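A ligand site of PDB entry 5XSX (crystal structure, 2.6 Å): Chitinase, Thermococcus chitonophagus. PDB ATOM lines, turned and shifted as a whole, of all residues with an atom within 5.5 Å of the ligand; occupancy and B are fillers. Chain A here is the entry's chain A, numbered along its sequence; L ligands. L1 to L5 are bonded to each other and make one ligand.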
ATOM      1  N   ASN A 174      19.819   6.059  33.739  1.00  0.00           N
ATOM      2  CA  ASN A 174      19.016   7.278  33.825  1.00  0.00           C
ATOM      3  C   ASN A 174      17.997   7.223  34.972  1.00  0.00           C
ATOM      4  O   ASN A 174      16.811   7.500  34.760  1.00  0.00           O
ATOM      5  CB  ASN A 174      18.293   7.527  32.502  1.00  0.00           C
ATOM      6  CG  ASN A 174      19.256   7.695  31.342  1.00  0.00           C
ATOM      7  OD1 ASN A 174      20.458   7.440  31.476  1.00  0.00           O
ATOM      8  ND2 ASN A 174      18.738   8.097  30.192  1.00  0.00           N
ATOM      9  N   LEU A 175      18.475   6.870  36.157  1.00  0.00           N
ATOM     10  CA  LEU A 175      17.654   6.768  37.360  1.00  0.00           C
ATOM     11  C   LEU A 175      16.523   5.758  37.184  1.00  0.00           C
ATOM     12  O   LEU A 175      15.388   6.007  37.574  1.00  0.00           O
ATOM     13  CB  LEU A 175      17.076   8.134  37.738  1.00  0.00           C
ATOM     14  CG  LEU A 175      18.093   9.252  37.975  1.00  0.00           C
ATOM     15  CD1 LEU A 175      17.383  10.529  38.420  1.00  0.00           C
ATOM     16  CD2 LEU A 175      19.134   8.824  38.999  1.00  0.00           C
ATOM     17  N   LYS A 212      21.486   6.016  26.590  1.00  0.00           N
ATOM     18  CA  LYS A 212      21.765   7.063  27.566  1.00  0.00           C
ATOM     19  C   LYS A 212      21.207   8.412  27.122  1.00  0.00           C
ATOM     20  O   LYS A 212      20.705   9.183  27.934  1.00  0.00           O
ATOM     21  CB  LYS A 212      23.280   7.168  27.802  1.00  0.00           C
ATOM     22  CG  LYS A 212      23.698   8.387  28.619  1.00  0.00           C
ATOM     23  CD  LYS A 212      23.093   8.355  30.004  1.00  0.00           C
ATOM     24  CE  LYS A 212      23.313   9.668  30.739  1.00  0.00           C
ATOM     25  NZ  LYS A 212      22.606   9.700  32.044  1.00  0.00           N
ATOM     26  N   GLU A 213      21.290   8.689  25.827  1.00  0.00           N
ATOM     27  CA  GLU A 213      20.898   9.986  25.300  1.00  0.00           C
ATOM     28  C   GLU A 213      19.397  10.227  25.320  1.00  0.00           C
ATOM     29  O   GLU A 213      18.951  11.315  25.693  1.00  0.00           O
ATOM     30  CB  GLU A 213      21.421  10.154  23.874  1.00  0.00           C
ATOM     31  CG  GLU A 213      22.936  10.309  23.771  1.00  0.00           C
ATOM     32  CD  GLU A 213      23.450  11.592  24.407  1.00  0.00           C
ATOM     33  OE1 GLU A 213      24.665  11.675  24.662  1.00  0.00           O
ATOM     34  OE2 GLU A 213      22.634  12.511  24.649  1.00  0.00           O
ATOM     35  N   ASN A 214      18.611   9.224  24.948  1.00  0.00           N
ATOM     36  CA  ASN A 214      17.165   9.406  24.831  1.00  0.00           C
ATOM     37  C   ASN A 214      16.378   8.099  24.815  1.00  0.00           C
ATOM     38  O   ASN A 214      15.335   8.010  24.175  1.00  0.00           O
ATOM     39  CB  ASN A 214      16.848  10.224  23.569  1.00  0.00           C
ATOM     40  CG  ASN A 214      15.451  10.815  23.593  1.00  0.00           C
ATOM     41  OD1 ASN A 214      14.824  10.943  24.644  1.00  0.00           O
ATOM     42  ND2 ASN A 214      14.952  11.180  22.410  1.00  0.00           N
ATOM     43  N   TRP A 215      16.880   7.093  25.519  1.00  0.00           N
ATOM     44  CA  TRP A 215      16.231   5.786  25.597  1.00  0.00           C
ATOM     45  C   TRP A 215      15.897   5.204  24.223  1.00  0.00           C
ATOM     46  O   TRP A 215      14.896   4.513  24.059  1.00  0.00           O
ATOM     47  CB  TRP A 215      14.941   5.870  26.428  1.00  0.00           C
ATOM     48  CG  TRP A 215      15.157   6.009  27.899  1.00  0.00           C
ATOM     49  CD1 TRP A 215      15.177   7.174  28.618  1.00  0.00           C
ATOM     50  CD2 TRP A 215      15.367   4.949  28.841  1.00  0.00           C
ATOM     51  NE1 TRP A 215      15.394   6.903  29.946  1.00  0.00           N
ATOM     52  CE2 TRP A 215      15.518   5.545  30.103  1.00  0.00           C
ATOM     53  CE3 TRP A 215      15.451   3.557  28.734  1.00  0.00           C
ATOM     54  CZ2 TRP A 215      15.740   4.798  31.262  1.00  0.00           C
ATOM     55  CZ3 TRP A 215      15.669   2.814  29.872  1.00  0.00           C
ATOM     56  CH2 TRP A 215      15.817   3.430  31.125  1.00  0.00           C
ATOM     57  N   PHE A 225       8.848   4.929  35.197  1.00  0.00           N
ATOM     58  CA  PHE A 225       9.028   5.441  33.842  1.00  0.00           C
ATOM     59  C   PHE A 225       7.833   5.147  32.949  1.00  0.00           C
ATOM     60  O   PHE A 225       7.452   3.996  32.773  1.00  0.00           O
ATOM     61  CB  PHE A 225      10.295   4.861  33.223  1.00  0.00           C
ATOM     62  CG  PHE A 225      11.554   5.574  33.612  1.00  0.00           C
ATOM     63  CD1 PHE A 225      12.249   5.207  34.745  1.00  0.00           C
ATOM     64  CD2 PHE A 225      12.026   6.634  32.850  1.00  0.00           C
ATOM     65  CE1 PHE A 225      13.398   5.876  35.114  1.00  0.00           C
ATOM     66  CE2 PHE A 225      13.175   7.302  33.218  1.00  0.00           C
ATOM     67  CZ  PHE A 225      13.860   6.926  34.346  1.00  0.00           C
ATOM     68  N   PRO A 240      10.648   4.747  27.151  1.00  0.00           N
ATOM     69  CA  PRO A 240      10.559   6.173  27.442  1.00  0.00           C
ATOM     70  C   PRO A 240      11.437   7.032  26.536  1.00  0.00           C
ATOM     71  O   PRO A 240      12.349   7.704  27.019  1.00  0.00           O
ATOM     72  CB  PRO A 240      11.020   6.262  28.889  1.00  0.00           C
ATOM     73  CG  PRO A 240      12.001   5.148  29.023  1.00  0.00           C
ATOM     74  CD  PRO A 240      11.551   4.048  28.087  1.00  0.00           C
ATOM     75  N   GLN A 242      11.781  10.210  23.868  1.00  0.00           N
ATOM     76  CA  GLN A 242      11.191  11.415  23.317  1.00  0.00           C
ATOM     77  C   GLN A 242      11.265  11.358  21.800  1.00  0.00           C
ATOM     78  O   GLN A 242      12.163  11.922  21.189  1.00  0.00           O
ATOM     79  CB  GLN A 242      11.906  12.662  23.849  1.00  0.00           C
ATOM     80  CG  GLN A 242      12.100  12.674  25.354  1.00  0.00           C
ATOM     81  CD  GLN A 242      10.792  12.741  26.125  1.00  0.00           C
ATOM     82  OE1 GLN A 242       9.787  13.246  25.619  1.00  0.00           O
ATOM     83  NE2 GLN A 242      10.803  12.239  27.349  1.00  0.00           N
ATOM     84  N   HIS A 245      11.766  14.481  19.555  1.00  0.00           N
ATOM     85  CA  HIS A 245      12.976  15.283  19.703  1.00  0.00           C
ATOM     86  C   HIS A 245      13.736  15.392  18.378  1.00  0.00           C
ATOM     87  O   HIS A 245      14.141  14.384  17.807  1.00  0.00           O
ATOM     88  CB  HIS A 245      13.892  14.695  20.788  1.00  0.00           C
ATOM     89  CG  HIS A 245      14.811  15.691  21.408  1.00  0.00           C
ATOM     90  ND1 HIS A 245      15.711  16.436  20.680  1.00  0.00           N
ATOM     91  CD2 HIS A 245      14.970  16.076  22.697  1.00  0.00           C
ATOM     92  CE1 HIS A 245      16.388  17.228  21.485  1.00  0.00           C
ATOM     93  NE2 HIS A 245      15.960  17.030  22.721  1.00  0.00           N
ATOM     94  N   PHE A 250      20.037   9.951  19.335  1.00  0.00           N
ATOM     95  CA  PHE A 250      21.455  10.116  19.642  1.00  0.00           C
ATOM     96  C   PHE A 250      21.728  11.509  20.192  1.00  0.00           C
ATOM     97  O   PHE A 250      22.837  11.815  20.636  1.00  0.00           O
ATOM     98  CB  PHE A 250      22.308   9.866  18.401  1.00  0.00           C
ATOM     99  CG  PHE A 250      22.320   8.441  17.949  1.00  0.00           C
ATOM    100  CD1 PHE A 250      23.125   7.500  18.563  1.00  0.00           C
ATOM    101  CD2 PHE A 250      21.499   8.034  16.899  1.00  0.00           C
ATOM    102  CE1 PHE A 250      23.131   6.186  18.148  1.00  0.00           C
ATOM    103  CE2 PHE A 250      21.504   6.712  16.478  1.00  0.00           C
ATOM    104  CZ  PHE A 250      22.320   5.788  17.103  1.00  0.00           C
ATOM    105  N   GLN A 251      20.694  12.357  20.173  1.00  0.00           N
ATOM    106  CA  GLN A 251      20.786  13.728  20.659  1.00  0.00           C
ATOM    107  C   GLN A 251      21.925  14.494  19.979  1.00  0.00           C
ATOM    108  O   GLN A 251      22.719  15.144  20.655  1.00  0.00           O
ATOM    109  CB  GLN A 251      20.949  13.758  22.173  1.00  0.00           C
ATOM    110  CG  GLN A 251      19.717  13.319  22.941  1.00  0.00           C
ATOM    111  CD  GLN A 251      18.527  14.230  22.699  1.00  0.00           C
ATOM    112  OE1 GLN A 251      18.678  15.447  22.569  1.00  0.00           O
ATOM    113  NE2 GLN A 251      17.336  13.646  22.628  1.00  0.00           N
ATOM    114  N   VAL A 252      21.994  14.408  18.661  1.00  0.00           N
ATOM    115  CA  VAL A 252      22.980  15.153  17.898  1.00  0.00           C
ATOM    116  C   VAL A 252      22.489  16.578  17.664  1.00  0.00           C
ATOM    117  O   VAL A 252      21.528  16.796  16.922  1.00  0.00           O
ATOM    118  CB  VAL A 252      23.279  14.483  16.541  1.00  0.00           C
ATOM    119  CG1 VAL A 252      24.198  15.370  15.712  1.00  0.00           C
ATOM    120  CG2 VAL A 252      23.892  13.114  16.749  1.00  0.00           C
ATOM    121  N   GLU A 253      23.149  17.543  18.299  1.00  0.00           N
ATOM    122  CA  GLU A 253      22.748  18.938  18.214  1.00  0.00           C
ATOM    123  C   GLU A 253      22.904  19.476  16.795  1.00  0.00           C
ATOM    124  O   GLU A 253      23.659  18.932  15.996  1.00  0.00           O
ATOM    125  CB  GLU A 253      23.558  19.795  19.193  1.00  0.00           C
ATOM    126  CG  GLU A 253      23.277  19.510  20.649  1.00  0.00           C
ATOM    127  CD  GLU A 253      24.126  20.340  21.596  1.00  0.00           C
ATOM    128  OE1 GLU A 253      25.125  20.932  21.125  1.00  0.00           O
ATOM    129  OE2 GLU A 253      23.807  20.396  22.797  1.00  0.00           O
ATOM    130  N   GLY A 255      24.261  22.243  15.859  1.00  0.00           N
ATOM    131  CA  GLY A 255      25.585  22.816  15.681  1.00  0.00           C
ATOM    132  C   GLY A 255      26.638  21.769  15.370  1.00  0.00           C
ATOM    133  O   GLY A 255      27.530  21.995  14.559  1.00  0.00           O
ATOM    134  N   ASN A 256      26.525  20.614  16.019  1.00  0.00           N
ATOM    135  CA  ASN A 256      27.452  19.516  15.777  1.00  0.00           C
ATOM    136  C   ASN A 256      27.225  18.883  14.401  1.00  0.00           C
ATOM    137  O   ASN A 256      28.166  18.437  13.749  1.00  0.00           O
ATOM    138  CB  ASN A 256      27.320  18.457  16.871  1.00  0.00           C
ATOM    139  CG  ASN A 256      28.294  17.300  16.688  1.00  0.00           C
ATOM    140  OD1 ASN A 256      27.978  16.312  16.026  1.00  0.00           O
ATOM    141  ND2 ASN A 256      29.468  17.422  17.282  1.00  0.00           N
ATOM    142  N   GLN A 259      28.618  21.133  11.660  1.00  0.00           N
ATOM    143  CA  GLN A 259      30.066  21.172  11.755  1.00  0.00           C
ATOM    144  C   GLN A 259      30.711  19.992  11.040  1.00  0.00           C
ATOM    145  O   GLN A 259      31.633  20.152  10.247  1.00  0.00           O
ATOM    146  CB  GLN A 259      30.516  21.211  13.218  1.00  0.00           C
ATOM    147  CG  GLN A 259      32.013  21.424  13.413  1.00  0.00           C
ATOM    148  CD  GLN A 259      32.468  22.824  13.027  1.00  0.00           C
ATOM    149  OE1 GLN A 259      32.550  23.709  13.874  1.00  0.00           O
ATOM    150  NE2 GLN A 259      32.778  23.009  11.746  1.00  0.00           N
ATOM    151  N   SER A 299      30.088  11.761  13.466  1.00  0.00           N
ATOM    152  CA  SER A 299      30.345  12.740  14.512  1.00  0.00           C
ATOM    153  C   SER A 299      31.319  12.198  15.554  1.00  0.00           C
ATOM    154  O   SER A 299      32.187  12.924  16.051  1.00  0.00           O
ATOM    155  CB  SER A 299      29.043  13.172  15.192  1.00  0.00           C
ATOM    156  OG  SER A 299      29.297  14.048  16.273  1.00  0.00           O
ATOM    157  N   GLY A 335      33.885  13.440  24.884  1.00  0.00           N
ATOM    158  CA  GLY A 335      33.902  14.503  23.901  1.00  0.00           C
ATOM    159  C   GLY A 335      32.594  14.603  23.139  1.00  0.00           C
ATOM    160  O   GLY A 335      32.240  15.654  22.617  1.00  0.00           O
ATOM    161  N   TYR A 336      31.879  13.492  23.066  1.00  0.00           N
ATOM    162  CA  TYR A 336      30.579  13.475  22.405  1.00  0.00           C
ATOM    163  C   TYR A 336      29.572  14.287  23.207  1.00  0.00           C
ATOM    164  O   TYR A 336      28.822  15.084  22.647  1.00  0.00           O
ATOM    165  CB  TYR A 336      30.086  12.036  22.225  1.00  0.00           C
ATOM    166  CG  TYR A 336      28.797  11.928  21.437  1.00  0.00           C
ATOM    167  CD1 TYR A 336      28.805  11.912  20.047  1.00  0.00           C
ATOM    168  CD2 TYR A 336      27.580  11.822  22.087  1.00  0.00           C
ATOM    169  CE1 TYR A 336      27.638  11.805  19.320  1.00  0.00           C
ATOM    170  CE2 TYR A 336      26.393  11.712  21.364  1.00  0.00           C
ATOM    171  CZ  TYR A 336      26.433  11.709  19.988  1.00  0.00           C
ATOM    172  OH  TYR A 336      25.268  11.604  19.276  1.00  0.00           O
ATOM    173  N   ASN A 337      29.586  14.083  24.522  1.00  0.00           N
ATOM    174  CA  ASN A 337      28.617  14.736  25.397  1.00  0.00           C
ATOM    175  C   ASN A 337      28.998  16.165  25.753  1.00  0.00           C
ATOM    176  O   ASN A 337      28.152  17.059  25.736  1.00  0.00           O
ATOM    177  CB  ASN A 337      28.448  13.916  26.674  1.00  0.00           C
ATOM    178  CG  ASN A 337      27.437  14.522  27.627  1.00  0.00           C
ATOM    179  OD1 ASN A 337      27.787  15.190  28.598  1.00  0.00           O
ATOM    180  ND2 ASN A 337      26.153  14.284  27.345  1.00  0.00           N
ATOM    181  N   ARG A 338      30.270  16.385  26.075  1.00  0.00           N
ATOM    182  CA  ARG A 338      30.724  17.686  26.545  1.00  0.00           C
ATOM    183  C   ARG A 338      31.291  18.568  25.438  1.00  0.00           C
ATOM    184  O   ARG A 338      31.330  19.792  25.562  1.00  0.00           O
ATOM    185  CB  ARG A 338      31.768  17.517  27.643  1.00  0.00           C
ATOM    186  CG  ARG A 338      31.215  17.003  28.960  1.00  0.00           C
ATOM    187  CD  ARG A 338      30.311  18.035  29.611  1.00  0.00           C
ATOM    188  NE  ARG A 338      29.964  17.668  30.979  1.00  0.00           N
ATOM    189  CZ  ARG A 338      30.699  17.959  32.050  1.00  0.00           C
ATOM    190  NH1 ARG A 338      31.823  18.646  31.908  1.00  0.00           N
ATOM    191  NH2 ARG A 338      30.306  17.582  33.253  1.00  0.00           N
ATOM    192  N   GLY A 339      31.732  17.939  24.351  1.00  0.00           N
ATOM    193  CA  GLY A 339      32.337  18.677  23.249  1.00  0.00           C
ATOM    194  C   GLY A 339      33.807  18.339  23.095  1.00  0.00           C
ATOM    195  O   GLY A 339      34.425  17.787  24.010  1.00  0.00           O
ATOM    196  N   VAL A 340      34.376  18.664  21.937  1.00  0.00           N
ATOM    197  CA  VAL A 340      35.781  18.385  21.676  1.00  0.00           C
ATOM    198  C   VAL A 340      36.699  19.301  22.480  1.00  0.00           C
ATOM    199  O   VAL A 340      37.831  18.937  22.804  1.00  0.00           O
ATOM    200  CB  VAL A 340      36.120  18.528  20.172  1.00  0.00           C
ATOM    201  CG1 VAL A 340      35.548  17.364  19.385  1.00  0.00           C
ATOM    202  CG2 VAL A 340      35.610  19.860  19.637  1.00  0.00           C
ATOM    203  N   GLY A 341      36.193  20.491  22.805  1.00  0.00           N
ATOM    204  CA  GLY A 341      36.952  21.443  23.599  1.00  0.00           C
ATOM    205  C   GLY A 341      37.198  20.926  24.999  1.00  0.00           C
ATOM    206  O   GLY A 341      38.233  21.211  25.600  1.00  0.00           O
ATOM    207  N   ALA A 342      36.255  20.151  25.507  1.00  0.00           N
ATOM    208  CA  ALA A 342      36.376  19.545  26.828  1.00  0.00           C
ATOM    209  C   ALA A 342      37.542  18.575  26.887  1.00  0.00           C
ATOM    210  O   ALA A 342      38.319  18.586  27.844  1.00  0.00           O
ATOM    211  CB  ALA A 342      35.088  18.849  27.212  1.00  0.00           C
ATOM    212  N   PHE A 371      27.327  14.672  31.783  1.00  0.00           N
ATOM    213  CA  PHE A 371      25.993  15.006  32.264  1.00  0.00           C
ATOM    214  C   PHE A 371      25.182  13.752  32.569  1.00  0.00           C
ATOM    215  O   PHE A 371      24.945  12.922  31.688  1.00  0.00           O
ATOM    216  CB  PHE A 371      25.251  15.881  31.245  1.00  0.00           C
ATOM    217  CG  PHE A 371      25.579  17.343  31.368  1.00  0.00           C
ATOM    218  CD1 PHE A 371      26.733  17.858  30.797  1.00  0.00           C
ATOM    219  CD2 PHE A 371      24.728  18.204  32.040  1.00  0.00           C
ATOM    220  CE1 PHE A 371      27.030  19.205  30.902  1.00  0.00           C
ATOM    221  CE2 PHE A 371      25.015  19.551  32.147  1.00  0.00           C
ATOM    222  CZ  PHE A 371      26.171  20.052  31.577  1.00  0.00           C
ATOM    223  N   GLY A 372      24.759  13.620  33.817  1.00  0.00           N
ATOM    224  CA  GLY A 372      23.978  12.479  34.255  1.00  0.00           C
ATOM    225  C   GLY A 372      24.785  11.200  34.277  1.00  0.00           C
ATOM    226  O   GLY A 372      24.235  10.116  34.053  1.00  0.00           O
ATOM    227  N   GLY A 373      26.079  11.316  34.537  1.00  0.00           N
ATOM    228  CA  GLY A 373      26.968  10.174  34.530  1.00  0.00           C
ATOM    229  C   GLY A 373      27.027   9.543  33.161  1.00  0.00           C
ATOM    230  O   GLY A 373      26.904   8.329  33.027  1.00  0.00           O
ATOM    231  N   HIS A 374      27.205  10.371  32.134  1.00  0.00           N
ATOM    232  CA  HIS A 374      27.161   9.926  30.756  1.00  0.00           C
ATOM    233  C   HIS A 374      28.206   8.857  30.443  1.00  0.00           C
ATOM    234  O   HIS A 374      27.878   7.779  29.961  1.00  0.00           O
ATOM    235  CB  HIS A 374      27.353  11.123  29.809  1.00  0.00           C
ATOM    236  CG  HIS A 374      27.112  10.797  28.366  1.00  0.00           C
ATOM    237  ND1 HIS A 374      28.073  10.223  27.568  1.00  0.00           N
ATOM    238  CD2 HIS A 374      26.026  10.974  27.583  1.00  0.00           C
ATOM    239  CE1 HIS A 374      27.587  10.055  26.351  1.00  0.00           C
ATOM    240  NE2 HIS A 374      26.351  10.512  26.333  1.00  0.00           N
HETATM  241  C1  LIG L   1      17.287  11.073  32.915  1.00  0.00           C
HETATM  242  C2  LIG L   1      18.792  11.155  32.823  1.00  0.00           C
HETATM  243  C3  LIG L   1      19.247  11.882  31.609  1.00  0.00           C
HETATM  244  C4  LIG L   1      18.441  11.661  30.338  1.00  0.00           C
HETATM  245  C5  LIG L   1      16.999  11.207  30.498  1.00  0.00           C
HETATM  246  C6  LIG L   1      16.594  10.405  29.292  1.00  0.00           C
HETATM  247  C7  LIG L   1      20.317  11.219  34.829  1.00  0.00           C
HETATM  248  C8  LIG L   1      20.841  11.949  36.090  1.00  0.00           C
HETATM  249  N1  LIG L   1      19.288  11.836  34.002  1.00  0.00           N
HETATM  250  O1  LIG L   1      16.979  10.322  34.010  1.00  0.00           O
HETATM  251  O2  LIG L   1      20.629  11.497  31.322  1.00  0.00           O
HETATM  252  O3  LIG L   1      18.387  12.937  29.684  1.00  0.00           O
HETATM  253  O4  LIG L   1      16.745  10.404  31.706  1.00  0.00           O
HETATM  254  O5  LIG L   1      15.635  11.116  28.522  1.00  0.00           O
HETATM  255  O6  LIG L   1      20.773  10.140  34.525  1.00  0.00           O
HETATM  256  C1  LG2 L   2      19.188  12.966  28.493  1.00  0.00           C
HETATM  257  C2  LG2 L   2      18.702  14.134  27.680  1.00  0.00           C
HETATM  258  C3  LG2 L   2      19.642  14.552  26.606  1.00  0.00           C
HETATM  259  C4  LG2 L   2      20.988  14.791  27.145  1.00  0.00           C
HETATM  260  C5  LG2 L   2      21.517  13.530  27.783  1.00  0.00           C
HETATM  261  C6  LG2 L   2      22.877  13.766  28.342  1.00  0.00           C
HETATM  262  C7  LG2 L   2      16.394  14.817  26.993  1.00  0.00           C
HETATM  263  C8  LG2 L   2      15.039  14.431  26.366  1.00  0.00           C
HETATM  264  N1  LG2 L   2      17.417  13.818  27.091  1.00  0.00           N
HETATM  265  O1  LG2 L   2      19.144  15.770  26.004  1.00  0.00           O
HETATM  266  O2  LG2 L   2      21.887  15.226  26.082  1.00  0.00           O
HETATM  267  O3  LG2 L   2      20.616  13.069  28.879  1.00  0.00           O
HETATM  268  O4  LG2 L   2      23.348  12.594  29.000  1.00  0.00           O
HETATM  269  O5  LG2 L   2      16.584  15.950  27.423  1.00  0.00           O
HETATM  270  C1  LG3 L   3      22.775  16.230  25.704  1.00  0.00           C
HETATM  271  C2  LG3 L   3      23.677  17.337  26.168  1.00  0.00           C
HETATM  272  C3  LG3 L   3      24.344  18.029  25.041  1.00  0.00           C
HETATM  273  C4  LG3 L   3      25.057  17.100  24.103  1.00  0.00           C
HETATM  274  C5  LG3 L   3      24.170  15.929  23.688  1.00  0.00           C
HETATM  275  C6  LG3 L   3      24.987  14.929  22.967  1.00  0.00           C
HETATM  276  C7  LG3 L   3      22.918  18.264  28.439  1.00  0.00           C
HETATM  277  C8  LG3 L   3      22.107  19.285  29.279  1.00  0.00           C
HETATM  278  N1  LG3 L   3      22.893  18.328  26.964  1.00  0.00           N
HETATM  279  O1  LG3 L   3      25.288  18.978  25.592  1.00  0.00           O
HETATM  280  O2  LG3 L   3      25.453  17.821  22.899  1.00  0.00           O
HETATM  281  O3  LG3 L   3      23.521  15.268  24.822  1.00  0.00           O
HETATM  282  O4  LG3 L   3      25.817  14.226  23.893  1.00  0.00           O
HETATM  283  O5  LG3 L   3      23.571  17.412  28.992  1.00  0.00           O
HETATM  284  C1  LG4 L   4      26.827  18.096  22.888  1.00  0.00           C
HETATM  285  C2  LG4 L   4      27.252  18.308  21.456  1.00  0.00           C
HETATM  286  C3  LG4 L   4      28.538  19.048  21.276  1.00  0.00           C
HETATM  287  C4  LG4 L   4      28.698  20.222  22.174  1.00  0.00           C
HETATM  288  C5  LG4 L   4      28.417  19.843  23.620  1.00  0.00           C
HETATM  289  C6  LG4 L   4      28.532  21.023  24.496  1.00  0.00           C
HETATM  290  C7  LG4 L   4      26.459  16.545  19.849  1.00  0.00           C
HETATM  291  C8  LG4 L   4      26.627  15.161  19.196  1.00  0.00           C
HETATM  292  N1  LG4 L   4      27.407  16.998  20.838  1.00  0.00           N
HETATM  293  O1  LG4 L   4      28.599  19.500  19.904  1.00  0.00           O
HETATM  294  O2  LG4 L   4      30.061  20.713  22.051  1.00  0.00           O
HETATM  295  O3  LG4 L   4      27.074  19.285  23.764  1.00  0.00           O
HETATM  296  O4  LG4 L   4      27.815  22.129  23.912  1.00  0.00           O
HETATM  297  O5  LG4 L   4      25.511  17.255  19.517  1.00  0.00           O
HETATM  298  C1  LG5 L   5      30.070  22.021  21.549  1.00  0.00           C
HETATM  299  C2  LG5 L   5      31.458  22.565  21.617  1.00  0.00           C
HETATM  300  C3  LG5 L   5      31.547  23.931  21.023  1.00  0.00           C
HETATM  301  C4  LG5 L   5      30.978  23.993  19.644  1.00  0.00           C
HETATM  302  C5  LG5 L   5      29.583  23.412  19.575  1.00  0.00           C
HETATM  303  C6  LG5 L   5      29.136  23.383  18.132  1.00  0.00           C
HETATM  304  C7  LG5 L   5      33.134  22.060  23.420  1.00  0.00           C
HETATM  305  C8  LG5 L   5      33.575  22.122  24.903  1.00  0.00           C
HETATM  306  N1  LG5 L   5      31.864  22.628  23.018  1.00  0.00           N
HETATM  307  O1  LG5 L   5      32.934  24.311  20.975  1.00  0.00           O
HETATM  308  O2  LG5 L   5      30.919  25.372  19.215  1.00  0.00           O
HETATM  309  O3  LG5 L   5      29.529  22.055  20.141  1.00  0.00           O
HETATM  310  O4  LG5 L   5      29.545  22.185  17.526  1.00  0.00           O
HETATM  311  O5  LG5 L   5      33.869  21.522  22.565  1.00  0.00           O
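O5 of LG5 L5 is in hydrogen-bond range of N of Val 340 (3.0 Å). ND2 of Asn 174 lies close to O4 of LIG L1, at 3.4 Å. A nitrogen (N1) of LG4 L4 lies within hydrogen-bond range of the backbone carbonyl oxygen (O) of Tyr 336, 3.0 Å away. O1 of LG3 L3 lies close to O of Asn 337 (3.5 Å). The side-chain amide oxygen of Gln 251 is in hydrogen-bond range of an oxygen (O1) of LG2 L2, 3.5 Å away. The backbone carbonyl oxygen (O) of Phe 371 lies within hydrogen-bond range of an oxygen (O4) of LG2 L2 (3.1 Å). The side-chain amino group (NZ) of Lys 212 is in hydrogen-bond range of an oxygen (O2) of LIG L1 (2.8 Å). O4 of LG3 L3 lies close to ND2 of Asn 337. N of Glu 253 lies within hydrogen-bond range of O5 of LG4 L4, 2.7 Å away. The side-chain amide nitrogen (ND2) of Asn 256 sits close to an oxygen (O1) of LG4 L4 (3.5 Å). O5 of LG5 L5 is in hydrogen-bond range of N of Gly 341 (2.6 Å). O4 of LG3 L3 is in hydrogen-bond range of OE1 of Glu 213, 2.9 Å away. The backbone carbonyl oxygen of Asn 174 lies within hydrogen-bond range of an oxygen (O1) of LIG L1. OE2 of Glu 253 sits close to O1 of LG3 L3 (3.5 Å). The backbone carbonyl oxygen (O) of Glu 213 lies within hydrogen-bond range of a nitrogen (N1) of LG2 L2.
NE2 of Gln 251 lies close to ND2 of Asn 214 (3.4 Å). O of Gly 372 lies within hydrogen-bond range of NZ of Lys 212. The side-chain hydroxyl (OG) of Ser 299 sits at hydrogen-bond distance from the side-chain amide oxygen (OD1) of Asn 256 (2.6 Å). NE2 of His 374 is in hydrogen-bond range of OE1 of Glu 213. The side-chain amide oxygen (OD1) of Asn 337 sits at hydrogen-bond distance from the backbone NH (N) of Phe 371 (3.3 Å). The backbone carbonyl oxygen of Phe 250 is in hydrogen-bond range of the side-chain hydroxyl of Tyr 336 (2.8 Å). The side-chain amide oxygen (OD1) of Asn 174 sits close to the side-chain amino group (NZ) of Lys 212, 3.2 Å away. The side-chain amide nitrogen (ND2) of Asn 214 is in hydrogen-bond range of the backbone carbonyl oxygen (O) of Gln 242 (3.1 Å).
O of Gly 372 lies close to O6 of LIG L1, at 3.5 Å. Residues that only touch the ligand: Gly 339 (3.2 Å), Arg 338 (3.2 Å), Ala 342 (3.4 Å), His 374 (3.4 Å), Gln 242 (3.6 Å), Gly 255 (3.6 Å), Trp 215 (3.6 Å), Val 252 (3.6 Å) and Asn 214 (3.9 Å). Of the 30 residues printed, 21 come within 4 Å of the ligand.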
